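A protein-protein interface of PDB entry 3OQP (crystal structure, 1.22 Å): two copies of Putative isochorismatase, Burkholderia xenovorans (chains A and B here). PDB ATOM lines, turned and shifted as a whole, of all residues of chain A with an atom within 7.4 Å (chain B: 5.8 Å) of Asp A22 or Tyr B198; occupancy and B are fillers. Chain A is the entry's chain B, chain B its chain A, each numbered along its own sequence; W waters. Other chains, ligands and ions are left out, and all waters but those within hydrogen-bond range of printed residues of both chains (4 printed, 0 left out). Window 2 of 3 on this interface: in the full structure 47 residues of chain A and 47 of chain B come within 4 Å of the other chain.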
ATOM      1  N   ASN A  16      18.659 -14.255  34.554  1.00  0.00           N
ATOM      2  CA  ASN A  16      19.815 -13.761  33.806  1.00  0.00           C
ATOM      3  C   ASN A  16      20.628 -14.875  33.192  1.00  0.00           C
ATOM      4  O   ASN A  16      21.267 -14.665  32.166  1.00  0.00           O
ATOM      5  CB  ASN A  16      20.709 -12.918  34.700  1.00  0.00           C
ATOM      6  CG  ASN A  16      20.106 -11.586  35.082  1.00  0.00           C
ATOM      7  OD1 ASN A  16      19.353 -10.969  34.316  1.00  0.00           O
ATOM      8  ND2 ASN A  16      20.439 -11.120  36.277  1.00  0.00           N
ATOM      9  N   GLU A  17      20.625 -16.070  33.810  1.00  0.00           N
ATOM     10  CA  GLU A  17      21.392 -17.218  33.272  1.00  0.00           C
ATOM     11  C   GLU A  17      21.124 -17.460  31.805  1.00  0.00           C
ATOM     12  O   GLU A  17      21.989 -17.881  31.019  1.00  0.00           O
ATOM     13  CB  GLU A  17      21.074 -18.491  34.071  1.00  0.00           C
ATOM     14  CG  GLU A  17      22.145 -19.528  34.075  1.00  0.00           C
ATOM     15  CD  GLU A  17      23.347 -19.058  34.897  1.00  0.00           C
ATOM     16  OE1 GLU A  17      23.259 -19.176  36.129  1.00  0.00           O
ATOM     17  OE2 GLU A  17      24.351 -18.574  34.329  1.00  0.00           O
ATOM     18  N   TYR A  18      19.866 -17.229  31.408  1.00  0.00           N
ATOM     19  CA  TYR A  18      19.395 -17.454  30.076  1.00  0.00           C
ATOM     20  C   TYR A  18      19.737 -16.357  29.063  1.00  0.00           C
ATOM     21  O   TYR A  18      19.581 -16.556  27.878  1.00  0.00           O
ATOM     22  CB  TYR A  18      17.852 -17.626  30.102  1.00  0.00           C
ATOM     23  CG  TYR A  18      17.384 -18.924  30.687  1.00  0.00           C
ATOM     24  CD1 TYR A  18      17.755 -20.143  30.134  1.00  0.00           C
ATOM     25  CD2 TYR A  18      16.526 -18.965  31.772  1.00  0.00           C
ATOM     26  CE1 TYR A  18      17.282 -21.339  30.681  1.00  0.00           C
ATOM     27  CE2 TYR A  18      16.071 -20.148  32.279  1.00  0.00           C
ATOM     28  CZ  TYR A  18      16.450 -21.340  31.732  1.00  0.00           C
ATOM     29  OH  TYR A  18      16.070 -22.559  32.193  1.00  0.00           O
ATOM     30  N   VAL A  19      20.208 -15.216  29.566  1.00  0.00           N
ATOM     31  CA  VAL A  19      20.389 -14.017  28.755  1.00  0.00           C
ATOM     32  C   VAL A  19      21.870 -13.654  28.741  1.00  0.00           C
ATOM     33  O   VAL A  19      22.513 -13.670  27.656  1.00  0.00           O
ATOM     34  CB  VAL A  19      19.475 -12.879  29.255  1.00  0.00           C
ATOM     35  CG1 VAL A  19      19.592 -11.670  28.299  1.00  0.00           C
ATOM     36  CG2 VAL A  19      18.012 -13.376  29.389  1.00  0.00           C
ATOM     37  N   THR A  20      22.429 -13.322  29.901  1.00  0.00           N
ATOM     38  CA  THR A  20      23.840 -12.930  30.022  1.00  0.00           C
ATOM     39  C   THR A  20      24.714 -14.006  30.654  1.00  0.00           C
ATOM     40  O   THR A  20      25.960 -13.816  30.733  1.00  0.00           O
ATOM     41  CB  THR A  20      23.936 -11.653  30.840  1.00  0.00           C
ATOM     42  OG1 THR A  20      23.283 -11.810  32.123  1.00  0.00           O
ATOM     43  CG2 THR A  20      23.316 -10.486  30.075  1.00  0.00           C
ATOM     44  N   GLY A  21      24.085 -15.100  31.120  1.00  0.00           N
ATOM     45  CA  GLY A  21      24.756 -16.163  31.835  1.00  0.00           C
ATOM     46  C   GLY A  21      25.182 -17.331  30.982  1.00  0.00           C
ATOM     47  O   GLY A  21      25.342 -17.209  29.769  1.00  0.00           O
ATOM     48  N   ASP A  22      25.302 -18.493  31.622  1.00  0.00           N
ATOM     49  CA  ASP A  22      25.940 -19.648  31.008  1.00  0.00           C
ATOM     50  C   ASP A  22      24.948 -20.679  30.494  1.00  0.00           C
ATOM     51  O   ASP A  22      25.320 -21.838  30.284  1.00  0.00           O
ATOM     52  CB  ASP A  22      26.936 -20.286  32.027  1.00  0.00           C
ATOM     53  CG  ASP A  22      28.190 -20.892  31.386  1.00  0.00           C
ATOM     54  OD1 ASP A  22      28.359 -20.894  30.135  1.00  0.00           O
ATOM     55  OD2 ASP A  22      29.021 -21.368  32.220  1.00  0.00           O
ATOM     56  N   LEU A  23      23.673 -20.311  30.307  1.00  0.00           N
ATOM     57  CA  LEU A  23      22.683 -21.187  29.634  1.00  0.00           C
ATOM     58  C   LEU A  23      21.902 -20.345  28.622  1.00  0.00           C
ATOM     59  O   LEU A  23      20.690 -20.169  28.753  1.00  0.00           O
ATOM     60  CB  LEU A  23      21.772 -21.892  30.662  1.00  0.00           C
ATOM     61  CG  LEU A  23      20.865 -23.002  30.111  1.00  0.00           C
ATOM     62  CD1 LEU A  23      21.625 -24.101  29.416  1.00  0.00           C
ATOM     63  CD2 LEU A  23      20.013 -23.581  31.253  1.00  0.00           C
ATOM     64  N   PRO A  24      22.618 -19.841  27.584  1.00  0.00           N
ATOM     65  CA  PRO A  24      21.988 -18.815  26.739  1.00  0.00           C
ATOM     66  C   PRO A  24      20.929 -19.381  25.841  1.00  0.00           C
ATOM     67  O   PRO A  24      21.176 -20.291  25.073  1.00  0.00           O
ATOM     68  CB  PRO A  24      23.151 -18.219  25.936  1.00  0.00           C
ATOM     69  CG  PRO A  24      24.221 -19.141  26.060  1.00  0.00           C
ATOM     70  CD  PRO A  24      24.035 -19.980  27.269  1.00  0.00           C
ATOM     71  N   ILE A  25      19.729 -18.831  25.940  1.00  0.00           N
ATOM     72  CA  ILE A  25      18.687 -19.170  25.014  1.00  0.00           C
ATOM     73  C   ILE A  25      19.073 -18.847  23.583  1.00  0.00           C
ATOM     74  O   ILE A  25      19.596 -17.763  23.338  1.00  0.00           O
ATOM     75  CB  ILE A  25      17.422 -18.387  25.374  1.00  0.00           C
ATOM     76  CG1 ILE A  25      16.793 -18.869  26.693  1.00  0.00           C
ATOM     77  CG2 ILE A  25      16.367 -18.472  24.256  1.00  0.00           C
ATOM     78  CD1 ILE A  25      16.198 -20.287  26.751  1.00  0.00           C
ATOM     79  N   PRO A  63      26.910 -24.515  38.864  1.00  0.00           N
ATOM     80  CA  PRO A  63      27.255 -23.802  37.621  1.00  0.00           C
ATOM     81  C   PRO A  63      26.146 -22.947  37.059  1.00  0.00           C
ATOM     82  O   PRO A  63      26.422 -21.973  36.380  1.00  0.00           O
ATOM     83  CB  PRO A  63      27.616 -24.894  36.636  1.00  0.00           C
ATOM     84  CG  PRO A  63      27.277 -26.167  37.284  1.00  0.00           C
ATOM     85  CD  PRO A  63      27.110 -25.964  38.742  1.00  0.00           C
ATOM     86  N   LEU A  64      24.892 -23.318  37.325  1.00  0.00           N
ATOM     87  CA  LEU A  64      23.733 -22.611  36.745  1.00  0.00           C
ATOM     88  C   LEU A  64      22.708 -22.337  37.831  1.00  0.00           C
ATOM     89  O   LEU A  64      22.478 -23.181  38.695  1.00  0.00           O
ATOM     90  CB  LEU A  64      23.076 -23.429  35.625  1.00  0.00           C
ATOM     91  CG  LEU A  64      23.943 -23.802  34.409  1.00  0.00           C
ATOM     92  CD1 LEU A  64      23.154 -24.680  33.435  1.00  0.00           C
ATOM     93  CD2 LEU A  64      24.517 -22.577  33.654  1.00  0.00           C
ATOM     94  N   GLY A  71      23.380 -14.885  37.742  1.00  0.00           N
ATOM     95  CA  GLY A  71      22.611 -15.762  36.860  1.00  0.00           C
ATOM     96  C   GLY A  71      21.254 -16.179  37.399  1.00  0.00           C
ATOM     97  O   GLY A  71      20.314 -16.341  36.627  1.00  0.00           O
ATOM     98  N   VAL A 147      17.629 -24.133  24.146  1.00  0.00           N
ATOM     99  CA  VAL A 147      19.080 -24.126  23.965  1.00  0.00           C
ATOM    100  C   VAL A 147      19.370 -25.446  23.266  1.00  0.00           C
ATOM    101  O   VAL A 147      18.567 -26.382  23.298  1.00  0.00           O
ATOM    102  CB  VAL A 147      19.787 -24.091  25.313  1.00  0.00           C
ATOM    103  CG1 VAL A 147      19.273 -22.882  26.216  1.00  0.00           C
ATOM    104  CG2 VAL A 147      19.582 -25.369  26.070  1.00  0.00           C
ATOM    105  N   PRO A 148      20.554 -25.522  22.624  1.00  0.00           N
ATOM    106  CA  PRO A 148      20.968 -26.806  22.050  1.00  0.00           C
ATOM    107  C   PRO A 148      21.538 -27.742  23.072  1.00  0.00           C
ATOM    108  O   PRO A 148      22.119 -27.285  24.106  1.00  0.00           O
ATOM    109  CB  PRO A 148      22.077 -26.378  21.037  1.00  0.00           C
ATOM    110  CG  PRO A 148      22.746 -25.143  21.689  1.00  0.00           C
ATOM    111  CD  PRO A 148      21.494 -24.424  22.296  1.00  0.00           C
ATOM    112  N   TYR A 149      21.430 -29.057  22.790  1.00  0.00           N
ATOM    113  CA  TYR A 149      21.963 -30.075  23.651  1.00  0.00           C
ATOM    114  C   TYR A 149      22.745 -31.091  22.831  1.00  0.00           C
ATOM    115  O   TYR A 149      22.352 -31.422  21.718  1.00  0.00           O
ATOM    116  CB  TYR A 149      20.859 -30.837  24.380  1.00  0.00           C
ATOM    117  CG  TYR A 149      20.143 -30.165  25.481  1.00  0.00           C
ATOM    118  CD1 TYR A 149      20.687 -29.185  26.286  1.00  0.00           C
ATOM    119  CD2 TYR A 149      18.880 -30.627  25.826  1.00  0.00           C
ATOM    120  CE1 TYR A 149      20.020 -28.640  27.377  1.00  0.00           C
ATOM    121  CE2 TYR A 149      18.109 -30.054  26.883  1.00  0.00           C
ATOM    122  CZ  TYR A 149      18.725 -29.068  27.663  1.00  0.00           C
ATOM    123  OH  TYR A 149      18.022 -28.532  28.714  1.00  0.00           O
ATOM    124  N   GLU A 150      23.830 -31.596  23.409  1.00  0.00           N
ATOM    125  CA  GLU A 150      24.488 -32.810  22.925  1.00  0.00           C
ATOM    126  C   GLU A 150      24.900 -33.648  24.104  1.00  0.00           C
ATOM    127  O   GLU A 150      25.600 -33.153  25.013  1.00  0.00           O
ATOM    128  CB  GLU A 150      25.708 -32.454  22.041  1.00  0.00           C
ATOM    129  CG  GLU A 150      26.369 -33.682  21.459  1.00  0.00           C
ATOM    130  CD  GLU A 150      27.512 -33.385  20.493  1.00  0.00           C
ATOM    131  OE1 GLU A 150      27.646 -32.235  20.005  1.00  0.00           O
ATOM    132  OE2 GLU A 150      28.322 -34.336  20.296  1.00  0.00           O
ATOM    133  N   ASN B 196      23.149 -34.226  32.220  1.00  0.00           N
ATOM    134  CA  ASN B 196      22.731 -33.036  32.936  1.00  0.00           C
ATOM    135  C   ASN B 196      22.712 -31.860  31.987  1.00  0.00           C
ATOM    136  O   ASN B 196      23.263 -31.895  30.894  1.00  0.00           O
ATOM    137  CB  ASN B 196      23.561 -32.774  34.194  1.00  0.00           C
ATOM    138  CG  ASN B 196      24.986 -32.406  33.876  1.00  0.00           C
ATOM    139  OD1 ASN B 196      25.276 -31.235  33.630  1.00  0.00           O
ATOM    140  ND2 ASN B 196      25.869 -33.403  33.864  1.00  0.00           N
ATOM    141  N   ILE B 197      21.973 -30.826  32.344  1.00  0.00           N
ATOM    142  CA  ILE B 197      21.687 -29.730  31.420  1.00  0.00           C
ATOM    143  C   ILE B 197      22.899 -28.926  31.076  1.00  0.00           C
ATOM    144  O   ILE B 197      23.109 -28.594  29.913  1.00  0.00           O
ATOM    145  CB  ILE B 197      20.581 -28.829  32.056  1.00  0.00           C
ATOM    146  CG1 ILE B 197      19.240 -29.564  31.982  1.00  0.00           C
ATOM    147  CG2 ILE B 197      20.410 -27.491  31.336  1.00  0.00           C
ATOM    148  CD1 ILE B 197      18.044 -28.899  32.727  1.00  0.00           C
ATOM    149  N   TYR B 198      23.714 -28.636  32.097  1.00  0.00           N
ATOM    150  CA  TYR B 198      24.934 -27.863  31.844  1.00  0.00           C
ATOM    151  C   TYR B 198      25.882 -28.635  30.910  1.00  0.00           C
ATOM    152  O   TYR B 198      26.293 -28.060  29.903  1.00  0.00           O
ATOM    153  CB  TYR B 198      25.568 -27.385  33.149  1.00  0.00           C
ATOM    154  CG  TYR B 198      26.772 -26.440  33.024  1.00  0.00           C
ATOM    155  CD1 TYR B 198      26.611 -25.137  32.613  1.00  0.00           C
ATOM    156  CD2 TYR B 198      28.101 -26.869  33.300  1.00  0.00           C
ATOM    157  CE1 TYR B 198      27.714 -24.264  32.499  1.00  0.00           C
ATOM    158  CE2 TYR B 198      29.187 -26.003  33.205  1.00  0.00           C
ATOM    159  CZ  TYR B 198      28.971 -24.721  32.785  1.00  0.00           C
ATOM    160  OH  TYR B 198      29.980 -23.846  32.683  1.00  0.00           O
ATOM    161  N   ALA B 199      26.183 -29.911  31.182  1.00  0.00           N
ATOM    162  CA  ALA B 199      27.066 -30.688  30.292  1.00  0.00           C
ATOM    163  C   ALA B 199      26.475 -30.754  28.914  1.00  0.00           C
ATOM    164  O   ALA B 199      27.135 -30.673  27.922  1.00  0.00           O
ATOM    165  CB  ALA B 199      27.239 -32.097  30.846  1.00  0.00           C
ATOM    166  N   SER B 200      25.156 -30.947  28.821  1.00  0.00           N
ATOM    167  CA  SER B 200      24.539 -31.112  27.528  1.00  0.00           C
ATOM    168  C   SER B 200      24.614 -29.853  26.712  1.00  0.00           C
ATOM    169  O   SER B 200      24.857 -29.888  25.485  1.00  0.00           O
ATOM    170  CB  SER B 200      23.060 -31.509  27.664  1.00  0.00           C
ATOM    171  OG  SER B 200      22.895 -32.823  28.189  1.00  0.00           O
ATOM    172  N   ASN B 201      24.372 -28.722  27.341  1.00  0.00           N
ATOM    173  CA  ASN B 201      24.438 -27.484  26.608  1.00  0.00           C
ATOM    174  C   ASN B 201      25.876 -27.082  26.298  1.00  0.00           C
ATOM    175  O   ASN B 201      26.152 -26.633  25.192  1.00  0.00           O
ATOM    176  CB  ASN B 201      23.717 -26.378  27.378  1.00  0.00           C
ATOM    177  CG  ASN B 201      23.806 -25.023  26.713  1.00  0.00           C
ATOM    178  OD1 ASN B 201      24.383 -24.095  27.290  1.00  0.00           O
ATOM    179  ND2 ASN B 201      23.264 -24.889  25.503  1.00  0.00           N
ATOM    180  N   GLN B 202      26.798 -27.319  27.225  1.00  0.00           N
ATOM    181  CA  GLN B 202      28.240 -27.040  26.982  1.00  0.00           C
ATOM    182  C   GLN B 202      28.790 -27.824  25.814  1.00  0.00           C
ATOM    183  O   GLN B 202      29.546 -27.268  24.971  1.00  0.00           O
ATOM    184  CB  GLN B 202      29.040 -27.354  28.233  1.00  0.00           C
ATOM    185  CG  GLN B 202      28.876 -26.369  29.344  1.00  0.00           C
ATOM    186  CD  GLN B 202      29.336 -24.956  29.059  1.00  0.00           C
ATOM    187  OE1 GLN B 202      30.473 -24.746  28.667  1.00  0.00           O
ATOM    188  NE2 GLN B 202      28.458 -23.981  29.283  1.00  0.00           N
ATOM    189  N   LYS B 203      28.434 -29.099  25.710  1.00  0.00           N
ATOM    190  CA  LYS B 203      28.940 -29.939  24.643  1.00  0.00           C
ATOM    191  C   LYS B 203      28.459 -29.416  23.294  1.00  0.00           C
ATOM    192  O   LYS B 203      29.229 -29.336  22.301  1.00  0.00           O
ATOM    193  CB  LYS B 203      28.531 -31.391  24.873  1.00  0.00           C
ATOM    194  CG  LYS B 203      29.312 -32.403  24.024  1.00  0.00           C
ATOM    195  CD  LYS B 203      28.927 -33.830  24.375  1.00  0.00           C
ATOM    196  CE  LYS B 203      29.800 -34.887  23.714  1.00  0.00           C
ATOM    197  NZ  LYS B 203      29.124 -36.220  23.757  1.00  0.00           N
ATOM    198  N   ARG B 205      27.525 -26.333  22.579  1.00  0.00           N
ATOM    199  CA  ARG B 205      28.160 -25.050  22.314  1.00  0.00           C
ATOM    200  C   ARG B 205      29.634 -25.160  21.930  1.00  0.00           C
ATOM    201  O   ARG B 205      30.118 -24.337  21.128  1.00  0.00           O
ATOM    202  CB  ARG B 205      28.051 -24.143  23.482  1.00  0.00           C
ATOM    203  CG  ARG B 205      26.621 -23.622  23.646  1.00  0.00           C
ATOM    204  CD  ARG B 205      26.441 -23.092  25.008  1.00  0.00           C
ATOM    205  NE  ARG B 205      27.188 -21.868  25.288  1.00  0.00           N
ATOM    206  CZ  ARG B 205      27.326 -21.350  26.502  1.00  0.00           C
ATOM    207  NH1 ARG B 205      26.765 -21.949  27.563  1.00  0.00           N
ATOM    208  NH2 ARG B 205      28.007 -20.234  26.658  1.00  0.00           N
HETATM  209  O   HOH W   1      26.664 -34.013  27.516  1.00  0.00           O
HETATM  210  O   HOH W   2      25.451 -24.468  29.840  1.00  0.00           O
HETATM  211  O   HOH W   3      23.079 -22.205  24.429  1.00  0.00           O
HETATM  212  O   HOH W   4      27.970 -17.884  28.016  1.00  0.00           O
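The side-chain carboxylate of Asp A22 lies within hydrogen-bond range of the side-chain hydroxyl of Tyr B198 (2.7 Å). O of Ser B200 is in hydrogen-bond range of N of Glu A150 (2.9 Å). ND2 of Asn B201 sits at hydrogen-bond distance from O of Pro A148, at 3.0 Å. The side-chain amide nitrogen of Gln B202 is in hydrogen-bond range of the side-chain carboxylate of Asp A22, at 3.2 Å. The guanidinium group (NH1) of Arg B205 lies within salt-bridge range of the side-chain carboxylate (OD1) of Asp A22, 3.2 Å away.
The side-chain amide oxygen (OD1) of Asn B196 lies close to the backbone NH (N) of Tyr B198, at 3.4 Å. The backbone carbonyl oxygen of Asn B196 is in hydrogen-bond range of the side-chain hydroxyl of Ser B200 (2.9 Å). The side-chain amide oxygen of Asn B201 sits at hydrogen-bond distance from the guanidinium group of Arg B205. NH1 of Arg B205 sits close to NE2 of Gln B202 (3.2 Å). The side-chain carboxylate (OE2) of Glu A17 sits at hydrogen-bond distance from the backbone NH (N) of Asp A22, at 2.9 Å. The backbone carbonyl oxygen of Glu A17 lies within hydrogen-bond range of the backbone NH of Leu A23 (3.0 Å).
Among the printed residues, pairs that only touch across the chains: Pro A24 with Arg B205, Glu A150 with Lys B203, Tyr A149 with Ser B200, Leu A64 with Tyr B198, Leu A23 with Asn B201, Val A147 with Asn B201, Tyr A149 with Ile B197, Tyr A149 with Asn B201, Asp A22 with Asn B201, Pro A63 with Tyr B198 and Leu A23 with Ile B197.
Of the printed residues of chain A, Tyr B198 touches Asp A22 (2.7 Å), Pro A63 (3.9 Å) and Leu A64 (3.5 Å). Printed residues of chain B within 4 Å of Glu A150: Ser B200 and Lys B203. Of the printed residues of chain B, Pro A148 touches Asn B201. Of the printed residues of chain B, Tyr A149 touches Ile B197 (3.6 Å), Ser B200 (3.4 Å) and Asn B201 (3.9 Å). Printed residues of chain B within 4 Å of Pro A24: Arg B205 (3.4 Å). Gly A21 touches none of the printed residues of chain B. The nearest printed residue of chain B that does not touch Asp A22 is Ile B197 (7.1 Å). The nearest printed residue of chain A that does not touch Tyr B198 is Leu A23 (5.6 Å). The nearest printed residue of chain B that does not touch Pro A24 is Asn B201 (4.1 Å).
Printed residues of chain A that touch a printed residue of chain B: Asp A22, Leu A23, Pro A24, Pro A63, Leu A64, Val A147, Pro A148, Tyr A149 and Glu A150. Hydrophobic or aromatic side chains of chain B that line the printed part of chain A: Ile B197 and Tyr B198. Among the printed residues, 16 pairs touch across the chains.
No position is printed for both chains. Of the 16 pairs that touch across the chains among the printed residues, none has its exchanged pair printed and touching as well.
Water W2 lies within hydrogen-bond range of O of Asp A22, OD1 of Asn B201 and NE2 of Gln B202. Water W4 bridges the guanidinium group of Arg B205 (2.7 Å) and the backbone carbonyl oxygen of Gly A21 (3.2 Å). Water W3 lies within hydrogen-bond range of O of Pro A24 (2.8 Å) and ND2 of Asn B201 (2.9 Å). Water W1 lies within hydrogen-bond range of the backbone carbonyl oxygen (O) of Glu A150 (2.9 Å) and the backbone carbonyl oxygen (O) of Ala B199 (3.4 Å).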
